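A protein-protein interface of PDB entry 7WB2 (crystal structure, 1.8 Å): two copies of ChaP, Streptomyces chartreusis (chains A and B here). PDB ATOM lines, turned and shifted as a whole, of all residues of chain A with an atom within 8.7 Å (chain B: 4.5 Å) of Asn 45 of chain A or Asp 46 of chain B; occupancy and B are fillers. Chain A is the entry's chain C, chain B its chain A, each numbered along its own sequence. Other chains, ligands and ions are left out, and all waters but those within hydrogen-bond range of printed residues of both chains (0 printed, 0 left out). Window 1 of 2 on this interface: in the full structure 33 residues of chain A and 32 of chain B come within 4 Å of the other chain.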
ATOM      1  N   MET A   2       7.172  25.268  25.686  1.00  0.00           N
ATOM      2  CA  MET A   2       6.444  26.282  24.929  1.00  0.00           C
ATOM      3  C   MET A   2       4.966  25.930  24.825  1.00  0.00           C
ATOM      4  O   MET A   2       4.607  24.762  24.906  1.00  0.00           O
ATOM      5  CB  MET A   2       7.074  26.425  23.543  1.00  0.00           C
ATOM      6  CG  MET A   2       6.332  25.731  22.404  1.00  0.00           C
ATOM      7  SD  MET A   2       6.652  23.950  22.420  1.00  0.00           S
ATOM      8  CE  MET A   2       8.259  23.877  21.654  1.00  0.00           C
ATOM      9  N   VAL A   4       3.085  27.924  22.311  1.00  0.00           N
ATOM     10  CA  VAL A   4       2.628  28.450  21.029  1.00  0.00           C
ATOM     11  C   VAL A   4       2.330  27.304  20.080  1.00  0.00           C
ATOM     12  O   VAL A   4       3.116  26.361  19.968  1.00  0.00           O
ATOM     13  CB  VAL A   4       3.684  29.385  20.419  1.00  0.00           C
ATOM     14  CG1 VAL A   4       3.084  30.192  19.277  1.00  0.00           C
ATOM     15  CG2 VAL A   4       4.189  30.324  21.489  1.00  0.00           C
ATOM     16  N   GLU A   5       1.217  27.425  19.355  1.00  0.00           N
ATOM     17  CA  GLU A   5       0.788  26.431  18.380  1.00  0.00           C
ATOM     18  C   GLU A   5       0.839  27.000  16.966  1.00  0.00           C
ATOM     19  O   GLU A   5       0.636  28.198  16.746  1.00  0.00           O
ATOM     20  CB  GLU A   5      -0.634  25.952  18.690  1.00  0.00           C
ATOM     21  CG  GLU A   5      -0.807  25.563  20.148  1.00  0.00           C
ATOM     22  CD  GLU A   5      -2.153  24.962  20.453  1.00  0.00           C
ATOM     23  OE1 GLU A   5      -2.358  24.563  21.612  1.00  0.00           O
ATOM     24  OE2 GLU A   5      -3.000  24.894  19.535  1.00  0.00           O
ATOM     25  N   LEU A   6       1.119  26.124  16.004  1.00  0.00           N
ATOM     26  CA  LEU A   6       0.974  26.466  14.597  1.00  0.00           C
ATOM     27  C   LEU A   6      -0.482  26.216  14.223  1.00  0.00           C
ATOM     28  O   LEU A   6      -0.946  25.069  14.220  1.00  0.00           O
ATOM     29  CB  LEU A   6       1.932  25.646  13.737  1.00  0.00           C
ATOM     30  CG  LEU A   6       1.890  25.961  12.241  1.00  0.00           C
ATOM     31  CD1 LEU A   6       2.454  27.345  11.965  1.00  0.00           C
ATOM     32  CD2 LEU A   6       2.674  24.909  11.496  1.00  0.00           C
ATOM     33  N   ASN A   7      -1.209  27.286  13.928  1.00  0.00           N
ATOM     34  CA  ASN A   7      -2.646  27.175  13.711  1.00  0.00           C
ATOM     35  C   ASN A   7      -3.002  26.941  12.248  1.00  0.00           C
ATOM     36  O   ASN A   7      -3.950  26.202  11.957  1.00  0.00           O
ATOM     37  CB  ASN A   7      -3.363  28.423  14.225  1.00  0.00           C
ATOM     38  CG  ASN A   7      -4.846  28.346  14.014  1.00  0.00           C
ATOM     39  OD1 ASN A   7      -5.355  28.810  12.997  1.00  0.00           O
ATOM     40  ND2 ASN A   7      -5.561  27.739  14.972  1.00  0.00           N
ATOM     41  N   HIS A   8      -2.276  27.564  11.319  1.00  0.00           N
ATOM     42  CA  HIS A   8      -2.463  27.256   9.907  1.00  0.00           C
ATOM     43  C   HIS A   8      -1.222  27.688   9.138  1.00  0.00           C
ATOM     44  O   HIS A   8      -0.419  28.500   9.608  1.00  0.00           O
ATOM     45  CB  HIS A   8      -3.742  27.896   9.325  1.00  0.00           C
ATOM     46  CG  HIS A   8      -3.873  29.373   9.557  1.00  0.00           C
ATOM     47  ND1 HIS A   8      -4.497  29.903  10.668  1.00  0.00           N
ATOM     48  CD2 HIS A   8      -3.493  30.432   8.799  1.00  0.00           C
ATOM     49  CE1 HIS A   8      -4.483  31.223  10.588  1.00  0.00           C
ATOM     50  NE2 HIS A   8      -3.878  31.569   9.465  1.00  0.00           N
ATOM     51  N   LEU A  41      -7.433  22.216   4.372  1.00  0.00           N
ATOM     52  CA  LEU A  41      -7.320  20.836   4.822  1.00  0.00           C
ATOM     53  C   LEU A  41      -7.045  20.896   6.317  1.00  0.00           C
ATOM     54  O   LEU A  41      -5.963  21.319   6.733  1.00  0.00           O
ATOM     55  CB  LEU A  41      -6.199  20.115   4.072  1.00  0.00           C
ATOM     56  CG  LEU A  41      -5.929  18.674   4.466  1.00  0.00           C
ATOM     57  CD1 LEU A  41      -6.604  17.756   3.466  1.00  0.00           C
ATOM     58  CD2 LEU A  41      -4.421  18.417   4.500  1.00  0.00           C
ATOM     59  N   GLN A  42      -8.009  20.465   7.122  1.00  0.00           N
ATOM     60  CA  GLN A  42      -7.861  20.490   8.572  1.00  0.00           C
ATOM     61  C   GLN A  42      -7.295  19.159   9.048  1.00  0.00           C
ATOM     62  O   GLN A  42      -7.827  18.098   8.712  1.00  0.00           O
ATOM     63  CB  GLN A  42      -9.206  20.778   9.254  1.00  0.00           C
ATOM     64  CG  GLN A  42      -9.085  21.046  10.756  1.00  0.00           C
ATOM     65  CD  GLN A  42     -10.427  21.214  11.455  1.00  0.00           C
ATOM     66  OE1 GLN A  42     -10.549  21.999  12.396  1.00  0.00           O
ATOM     67  NE2 GLN A  42     -11.441  20.490  10.994  1.00  0.00           N
ATOM     68  N   LEU A  43      -6.225  19.222   9.837  1.00  0.00           N
ATOM     69  CA  LEU A  43      -5.640  18.047  10.470  1.00  0.00           C
ATOM     70  C   LEU A  43      -6.081  17.977  11.934  1.00  0.00           C
ATOM     71  O   LEU A  43      -6.765  18.868  12.451  1.00  0.00           O
ATOM     72  CB  LEU A  43      -4.113  18.065  10.351  1.00  0.00           C
ATOM     73  CG  LEU A  43      -3.518  17.888   8.934  1.00  0.00           C
ATOM     74  CD1 LEU A  43      -4.292  16.848   8.128  1.00  0.00           C
ATOM     75  CD2 LEU A  43      -3.455  19.209   8.186  1.00  0.00           C
ATOM     76  N   ALA A  44      -5.737  16.869  12.596  1.00  0.00           N
ATOM     77  CA  ALA A  44      -6.325  16.623  13.914  1.00  0.00           C
ATOM     78  C   ALA A  44      -5.712  17.478  15.016  1.00  0.00           C
ATOM     79  O   ALA A  44      -6.376  17.732  16.032  1.00  0.00           O
ATOM     80  CB  ALA A  44      -6.205  15.147  14.299  1.00  0.00           C
ATOM     81  N   ASN A  45      -4.463  17.905  14.857  1.00  0.00           N
ATOM     82  CA  ASN A  45      -3.753  18.600  15.928  1.00  0.00           C
ATOM     83  C   ASN A  45      -3.877  20.124  15.840  1.00  0.00           C
ATOM     84  O   ASN A  45      -2.879  20.838  15.905  1.00  0.00           O
ATOM     85  CB  ASN A  45      -2.292  18.143  15.969  1.00  0.00           C
ATOM     86  CG  ASN A  45      -1.579  18.219  14.600  1.00  0.00           C
ATOM     87  OD1 ASN A  45      -2.159  17.916  13.558  1.00  0.00           O
ATOM     88  ND2 ASN A  45      -0.291  18.568  14.629  1.00  0.00           N
ATOM     89  N   ASP A  46      -5.112  20.631  15.725  1.00  0.00           N
ATOM     90  CA  ASP A  46      -5.402  22.073  15.809  1.00  0.00           C
ATOM     91  C   ASP A  46      -4.601  22.864  14.773  1.00  0.00           C
ATOM     92  O   ASP A  46      -4.077  23.946  15.057  1.00  0.00           O
ATOM     93  CB  ASP A  46      -5.147  22.606  17.233  1.00  0.00           C
ATOM     94  CG  ASP A  46      -5.924  23.880  17.540  1.00  0.00           C
ATOM     95  OD1 ASP A  46      -6.701  24.315  16.665  1.00  0.00           O
ATOM     96  OD2 ASP A  46      -5.759  24.456  18.655  1.00  0.00           O
ATOM     97  N   VAL A  47      -4.519  22.326  13.556  1.00  0.00           N
ATOM     98  CA  VAL A  47      -3.754  22.951  12.478  1.00  0.00           C
ATOM     99  C   VAL A  47      -4.420  22.665  11.142  1.00  0.00           C
ATOM    100  O   VAL A  47      -5.001  21.598  10.931  1.00  0.00           O
ATOM    101  CB  VAL A  47      -2.288  22.449  12.461  1.00  0.00           C
ATOM    102  CG1 VAL A  47      -2.241  20.962  12.206  1.00  0.00           C
ATOM    103  CG2 VAL A  47      -1.488  23.177  11.400  1.00  0.00           C
ATOM    104  N   SER A  48      -4.349  23.633  10.232  1.00  0.00           N
ATOM    105  CA  SER A  48      -4.836  23.346   8.891  1.00  0.00           C
ATOM    106  C   SER A  48      -3.804  23.808   7.877  1.00  0.00           C
ATOM    107  O   SER A  48      -3.089  24.784   8.102  1.00  0.00           O
ATOM    108  CB  SER A  48      -6.174  24.039   8.596  1.00  0.00           C
ATOM    109  OG  SER A  48      -7.004  24.080   9.740  1.00  0.00           O
ATOM    110  N   ALA A  66       4.613  16.756   5.927  1.00  0.00           N
ATOM    111  CA  ALA A  66       4.636  15.421   6.515  1.00  0.00           C
ATOM    112  C   ALA A  66       3.445  15.204   7.427  1.00  0.00           C
ATOM    113  O   ALA A  66       3.153  16.048   8.277  1.00  0.00           O
ATOM    114  CB  ALA A  66       5.917  15.199   7.310  1.00  0.00           C
ATOM    115  N   PHE A  67       2.785  14.058   7.265  1.00  0.00           N
ATOM    116  CA  PHE A  67       1.614  13.692   8.041  1.00  0.00           C
ATOM    117  C   PHE A  67       1.913  12.463   8.887  1.00  0.00           C
ATOM    118  O   PHE A  67       2.470  11.475   8.392  1.00  0.00           O
ATOM    119  CB  PHE A  67       0.418  13.450   7.111  1.00  0.00           C
ATOM    120  CG  PHE A  67       0.091  14.642   6.268  1.00  0.00           C
ATOM    121  CD1 PHE A  67      -0.773  15.618   6.739  1.00  0.00           C
ATOM    122  CD2 PHE A  67       0.709  14.830   5.038  1.00  0.00           C
ATOM    123  CE1 PHE A  67      -1.051  16.751   5.980  1.00  0.00           C
ATOM    124  CE2 PHE A  67       0.445  15.949   4.276  1.00  0.00           C
ATOM    125  CZ  PHE A  67      -0.439  16.918   4.744  1.00  0.00           C
ATOM    126  N   LEU A  68       1.595  12.556  10.170  1.00  0.00           N
ATOM    127  CA  LEU A  68       1.732  11.441  11.095  1.00  0.00           C
ATOM    128  C   LEU A  68       0.387  10.733  11.138  1.00  0.00           C
ATOM    129  O   LEU A  68      -0.653  11.381  11.325  1.00  0.00           O
ATOM    130  CB  LEU A  68       2.141  11.935  12.488  1.00  0.00           C
ATOM    131  CG  LEU A  68       2.157  10.947  13.666  1.00  0.00           C
ATOM    132  CD1 LEU A  68       3.228   9.881  13.513  1.00  0.00           C
ATOM    133  CD2 LEU A  68       2.288  11.693  15.018  1.00  0.00           C
ATOM    134  N   MET A 122       4.031   9.063   7.717  1.00  0.00           N
ATOM    135  CA  MET A 122       4.932   8.420   8.662  1.00  0.00           C
ATOM    136  C   MET A 122       4.114   7.910   9.832  1.00  0.00           C
ATOM    137  O   MET A 122       3.095   8.503  10.172  1.00  0.00           O
ATOM    138  CB  MET A 122       6.001   9.409   9.123  1.00  0.00           C
ATOM    139  CG  MET A 122       5.404  10.644   9.788  1.00  0.00           C
ATOM    140  SD  MET A 122       6.622  11.889  10.249  1.00  0.00           S
ATOM    141  CE  MET A 122       7.245  11.247  11.795  1.00  0.00           C
ATOM    142  N   GLU B   5      -2.459  13.735  11.685  1.00  0.00           N
ATOM    143  CA  GLU B   5      -1.893  14.990  12.138  1.00  0.00           C
ATOM    144  C   GLU B   5      -0.899  15.533  11.120  1.00  0.00           C
ATOM    145  O   GLU B   5      -0.217  14.771  10.435  1.00  0.00           O
ATOM    146  CB  GLU B   5      -1.170  14.826  13.479  1.00  0.00           C
ATOM    147  CG  GLU B   5      -2.110  14.480  14.605  1.00  0.00           C
ATOM    148  CD  GLU B   5      -1.420  14.357  15.943  1.00  0.00           C
ATOM    149  OE1 GLU B   5      -0.270  14.813  16.065  1.00  0.00           O
ATOM    150  OE2 GLU B   5      -2.049  13.827  16.880  1.00  0.00           O
ATOM    151  N   LEU B   6      -0.791  16.859  11.057  1.00  0.00           N
ATOM    152  CA  LEU B   6       0.320  17.472  10.333  1.00  0.00           C
ATOM    153  C   LEU B   6       1.500  17.504  11.291  1.00  0.00           C
ATOM    154  O   LEU B   6       1.441  18.179  12.322  1.00  0.00           O
ATOM    155  CB  LEU B   6      -0.008  18.885   9.850  1.00  0.00           C
ATOM    156  CG  LEU B   6       1.234  19.636   9.342  1.00  0.00           C
ATOM    157  CD1 LEU B   6       1.789  18.951   8.089  1.00  0.00           C
ATOM    158  CD2 LEU B   6       0.971  21.132   9.086  1.00  0.00           C
ATOM    159  N   ASN B   7       2.554  16.740  10.985  1.00  0.00           N
ATOM    160  CA  ASN B   7       3.671  16.583  11.916  1.00  0.00           C
ATOM    161  C   ASN B   7       4.816  17.573  11.681  1.00  0.00           C
ATOM    162  O   ASN B   7       5.437  18.028  12.646  1.00  0.00           O
ATOM    163  CB  ASN B   7       4.241  15.164  11.840  1.00  0.00           C
ATOM    164  CG  ASN B   7       5.352  14.943  12.858  1.00  0.00           C
ATOM    165  OD1 ASN B   7       6.524  15.004  12.527  1.00  0.00           O
ATOM    166  ND2 ASN B   7       4.982  14.730  14.107  1.00  0.00           N
ATOM    167  N   GLN B  42      10.110  23.508  17.031  1.00  0.00           N
ATOM    168  CA  GLN B  42       8.997  22.715  17.538  1.00  0.00           C
ATOM    169  C   GLN B  42       7.913  23.646  18.073  1.00  0.00           C
ATOM    170  O   GLN B  42       8.214  24.591  18.803  1.00  0.00           O
ATOM    171  CB  GLN B  42       9.495  21.790  18.650  1.00  0.00           C
ATOM    172  CG  GLN B  42       8.430  20.921  19.297  1.00  0.00           C
ATOM    173  CD  GLN B  42       7.959  19.823  18.384  1.00  0.00           C
ATOM    174  OE1 GLN B  42       6.770  19.681  18.134  1.00  0.00           O
ATOM    175  NE2 GLN B  42       8.902  19.051  17.854  1.00  0.00           N
ATOM    176  N   LEU B  43       6.668  23.427  17.656  1.00  0.00           N
ATOM    177  CA  LEU B  43       5.528  24.112  18.253  1.00  0.00           C
ATOM    178  C   LEU B  43       4.786  23.158  19.195  1.00  0.00           C
ATOM    179  O   LEU B  43       5.029  21.953  19.212  1.00  0.00           O
ATOM    180  CB  LEU B  43       4.592  24.654  17.170  1.00  0.00           C
ATOM    181  CG  LEU B  43       5.064  25.887  16.387  1.00  0.00           C
ATOM    182  CD1 LEU B  43       5.751  26.888  17.322  1.00  0.00           C
ATOM    183  CD2 LEU B  43       5.995  25.477  15.223  1.00  0.00           C
ATOM    184  N   ALA B  44       3.842  23.714  19.969  1.00  0.00           N
ATOM    185  CA  ALA B  44       3.232  22.940  21.046  1.00  0.00           C
ATOM    186  C   ALA B  44       2.245  21.888  20.538  1.00  0.00           C
ATOM    187  O   ALA B  44       2.029  20.876  21.222  1.00  0.00           O
ATOM    188  CB  ALA B  44       2.529  23.874  22.028  1.00  0.00           C
ATOM    189  N   ASN B  45       1.619  22.104  19.384  1.00  0.00           N
ATOM    190  CA  ASN B  45       0.598  21.162  18.926  1.00  0.00           C
ATOM    191  C   ASN B  45       1.182  20.092  18.005  1.00  0.00           C
ATOM    192  O   ASN B  45       0.606  19.743  16.973  1.00  0.00           O
ATOM    193  CB  ASN B  45      -0.556  21.899  18.252  1.00  0.00           C
ATOM    194  CG  ASN B  45      -0.095  22.902  17.207  1.00  0.00           C
ATOM    195  OD1 ASN B  45       0.949  23.513  17.343  1.00  0.00           O
ATOM    196  ND2 ASN B  45      -0.915  23.112  16.194  1.00  0.00           N
ATOM    197  N   ASP B  46       2.300  19.513  18.439  1.00  0.00           N
ATOM    198  CA  ASP B  46       2.897  18.341  17.795  1.00  0.00           C
ATOM    199  C   ASP B  46       3.193  18.591  16.320  1.00  0.00           C
ATOM    200  O   ASP B  46       2.942  17.744  15.468  1.00  0.00           O
ATOM    201  CB  ASP B  46       2.000  17.107  17.964  1.00  0.00           C
ATOM    202  CG  ASP B  46       2.792  15.796  17.958  1.00  0.00           C
ATOM    203  OD1 ASP B  46       4.036  15.860  17.946  1.00  0.00           O
ATOM    204  OD2 ASP B  46       2.165  14.709  17.996  1.00  0.00           O
ATOM    205  N   VAL B  47       3.734  19.764  16.002  1.00  0.00           N
ATOM    206  CA  VAL B  47       4.089  20.074  14.622  1.00  0.00           C
ATOM    207  C   VAL B  47       5.352  20.920  14.654  1.00  0.00           C
ATOM    208  O   VAL B  47       5.531  21.757  15.544  1.00  0.00           O
ATOM    209  CB  VAL B  47       2.927  20.770  13.877  1.00  0.00           C
ATOM    210  CG1 VAL B  47       2.496  22.042  14.600  1.00  0.00           C
ATOM    211  CG2 VAL B  47       3.308  21.080  12.427  1.00  0.00           C
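Of chain B, only Glu 5 (3.2 Å), Leu 6 (2.9 Å), Asn 45 (2.8 Å), Asp 46 (3.4 Å) and Val 47 (3.97 Å) come within 4 Å of Asn 45 of chain A. Of chain A, only Asn 45 comes within 4 Å of Asp 46 of chain B. Asn 45 of chain B touches just these residues of chain A: Glu 5 (3.1 Å), Leu 6 (2.8 Å), Asn 45 (2.8 Å) and Asp 46 (3.5 Å). Of the printed residues of chain B, Asp 46 of chain A touches Asn 45 (3.5 Å). Printed residues of chain B within 4 Å of Glu 5 of chain A: Asn 45 (3.1 Å). Of the printed residues of chain A, Glu 5 of chain B touches Asn 45, Phe 67 and Leu 68. Printed residues of chain B within 4 Å of Leu 43 of chain A: Leu 6 (3.6 Å). His 8 of chain A touches none of the printed residues of chain B. Ala 44 of chain A touches none of the printed residues of chain B. The nearest printed residue of chain B that does not touch Asn 45 of chain A is Asn 7 of chain B (5.0 Å).
Met 2 of chain A touches Gln 42 of chain B (CE to O, 2.9 Å). C of Leu 43 of chain B touches SD of Met 2 of chain A, 3.8 Å away. Leu 43 of chain B touches Val 4 of chain A (CB to O, 3.6 Å). Glu 5 of chain A touches Asn 45 of chain B (CA to OD1, 3.1 Å). N of Leu 6 of chain A touches CB of Leu 43 of chain B, 3.9 Å away. Leu 43 of chain A touches Leu 6 of chain B. Asn 45 of chain A touches Glu 5 of chain B (OD1 to CB, 3.2 Å). CB of Val 47 of chain B touches ND2 of Asn 45 of chain A, 3.97 Å away. Ala 66 of chain A touches Leu 6 of chain B (O to CD1, 3.2 Å). Glu 5 of chain B touches Phe 67 of chain A (O to CA, 3.2 Å).
The backbone carbonyl oxygen (O) of Phe 67 of chain A sits at hydrogen-bond distance from the backbone NH (N) of Met 122 of chain A, at 3.0 Å.
Glu 5 of chain A touches Asn 45 of chain B, and with the chains exchanged Asn 45 of chain A touches Glu 5 of chain B. Leu 6 of chain A touches Leu 43 of chain B, and with the chains exchanged Leu 43 of chain A touches Leu 6 of chain B. Leu 6 of chain A touches Asn 45 of chain B, and with the chains exchanged Asn 45 of chain A touches Leu 6 of chain B. Asn 45 of chain A touches Val 47 of chain B, but with the chains exchanged Val 47 of chain A does not touch Asn 45 of chain B (4.03 Å). Positions printed for both chains: 5, 6, 7, 42, 43, 44, 45, 46 and 47.
Hydrophobic or aromatic side chains of chain B that line the printed part of chain A: Leu 6, Leu 43, Ala 44 and Val 47. Hydrophobic or aromatic side chains of chain A within 4 Å of the printed part of chain B: Met 2, Leu 6, Leu 43, Val 47, Phe 67, Leu 68 and Met 122.
The backbone carbonyl oxygen (O) of Glu 5 of chain B is in hydrogen-bond range of the backbone NH (N) of Leu 68 of chain A (2.9 Å). The side-chain amide nitrogen (ND2) of Asn 45 of chain A sits at hydrogen-bond distance from the backbone carbonyl oxygen (O) of Leu 6 of chain B, at 2.9 Å. The backbone NH (N) of Asn 7 of chain B is in hydrogen-bond range of the backbone carbonyl oxygen (O) of Ala 66 of chain A, at 2.9 Å. N of Ala 44 of chain B lies within hydrogen-bond range of SD of Met 2 of chain A, 3.7 Å away. The backbone NH (N) of Ala 44 of chain B lies within hydrogen-bond range of the backbone carbonyl oxygen (O) of Val 4 of chain A (2.7 Å). ND2 of Asn 45 of chain B sits at hydrogen-bond distance from O of Leu 6 of chain A, 2.8 Å away. The backbone carbonyl oxygen of Asn 45 of chain B lies within hydrogen-bond range of the side-chain amide nitrogen of Asn 45 of chain A (2.8 Å). The backbone carbonyl oxygen (O) of Asp 46 of chain A lies within hydrogen-bond range of the side-chain amide nitrogen (ND2) of Asn 45 of chain B. The backbone carbonyl oxygen (O) of Asp 46 of chain B lies within hydrogen-bond range of the side-chain amide nitrogen (ND2) of Asn 45 of chain A, 3.4 Å away.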
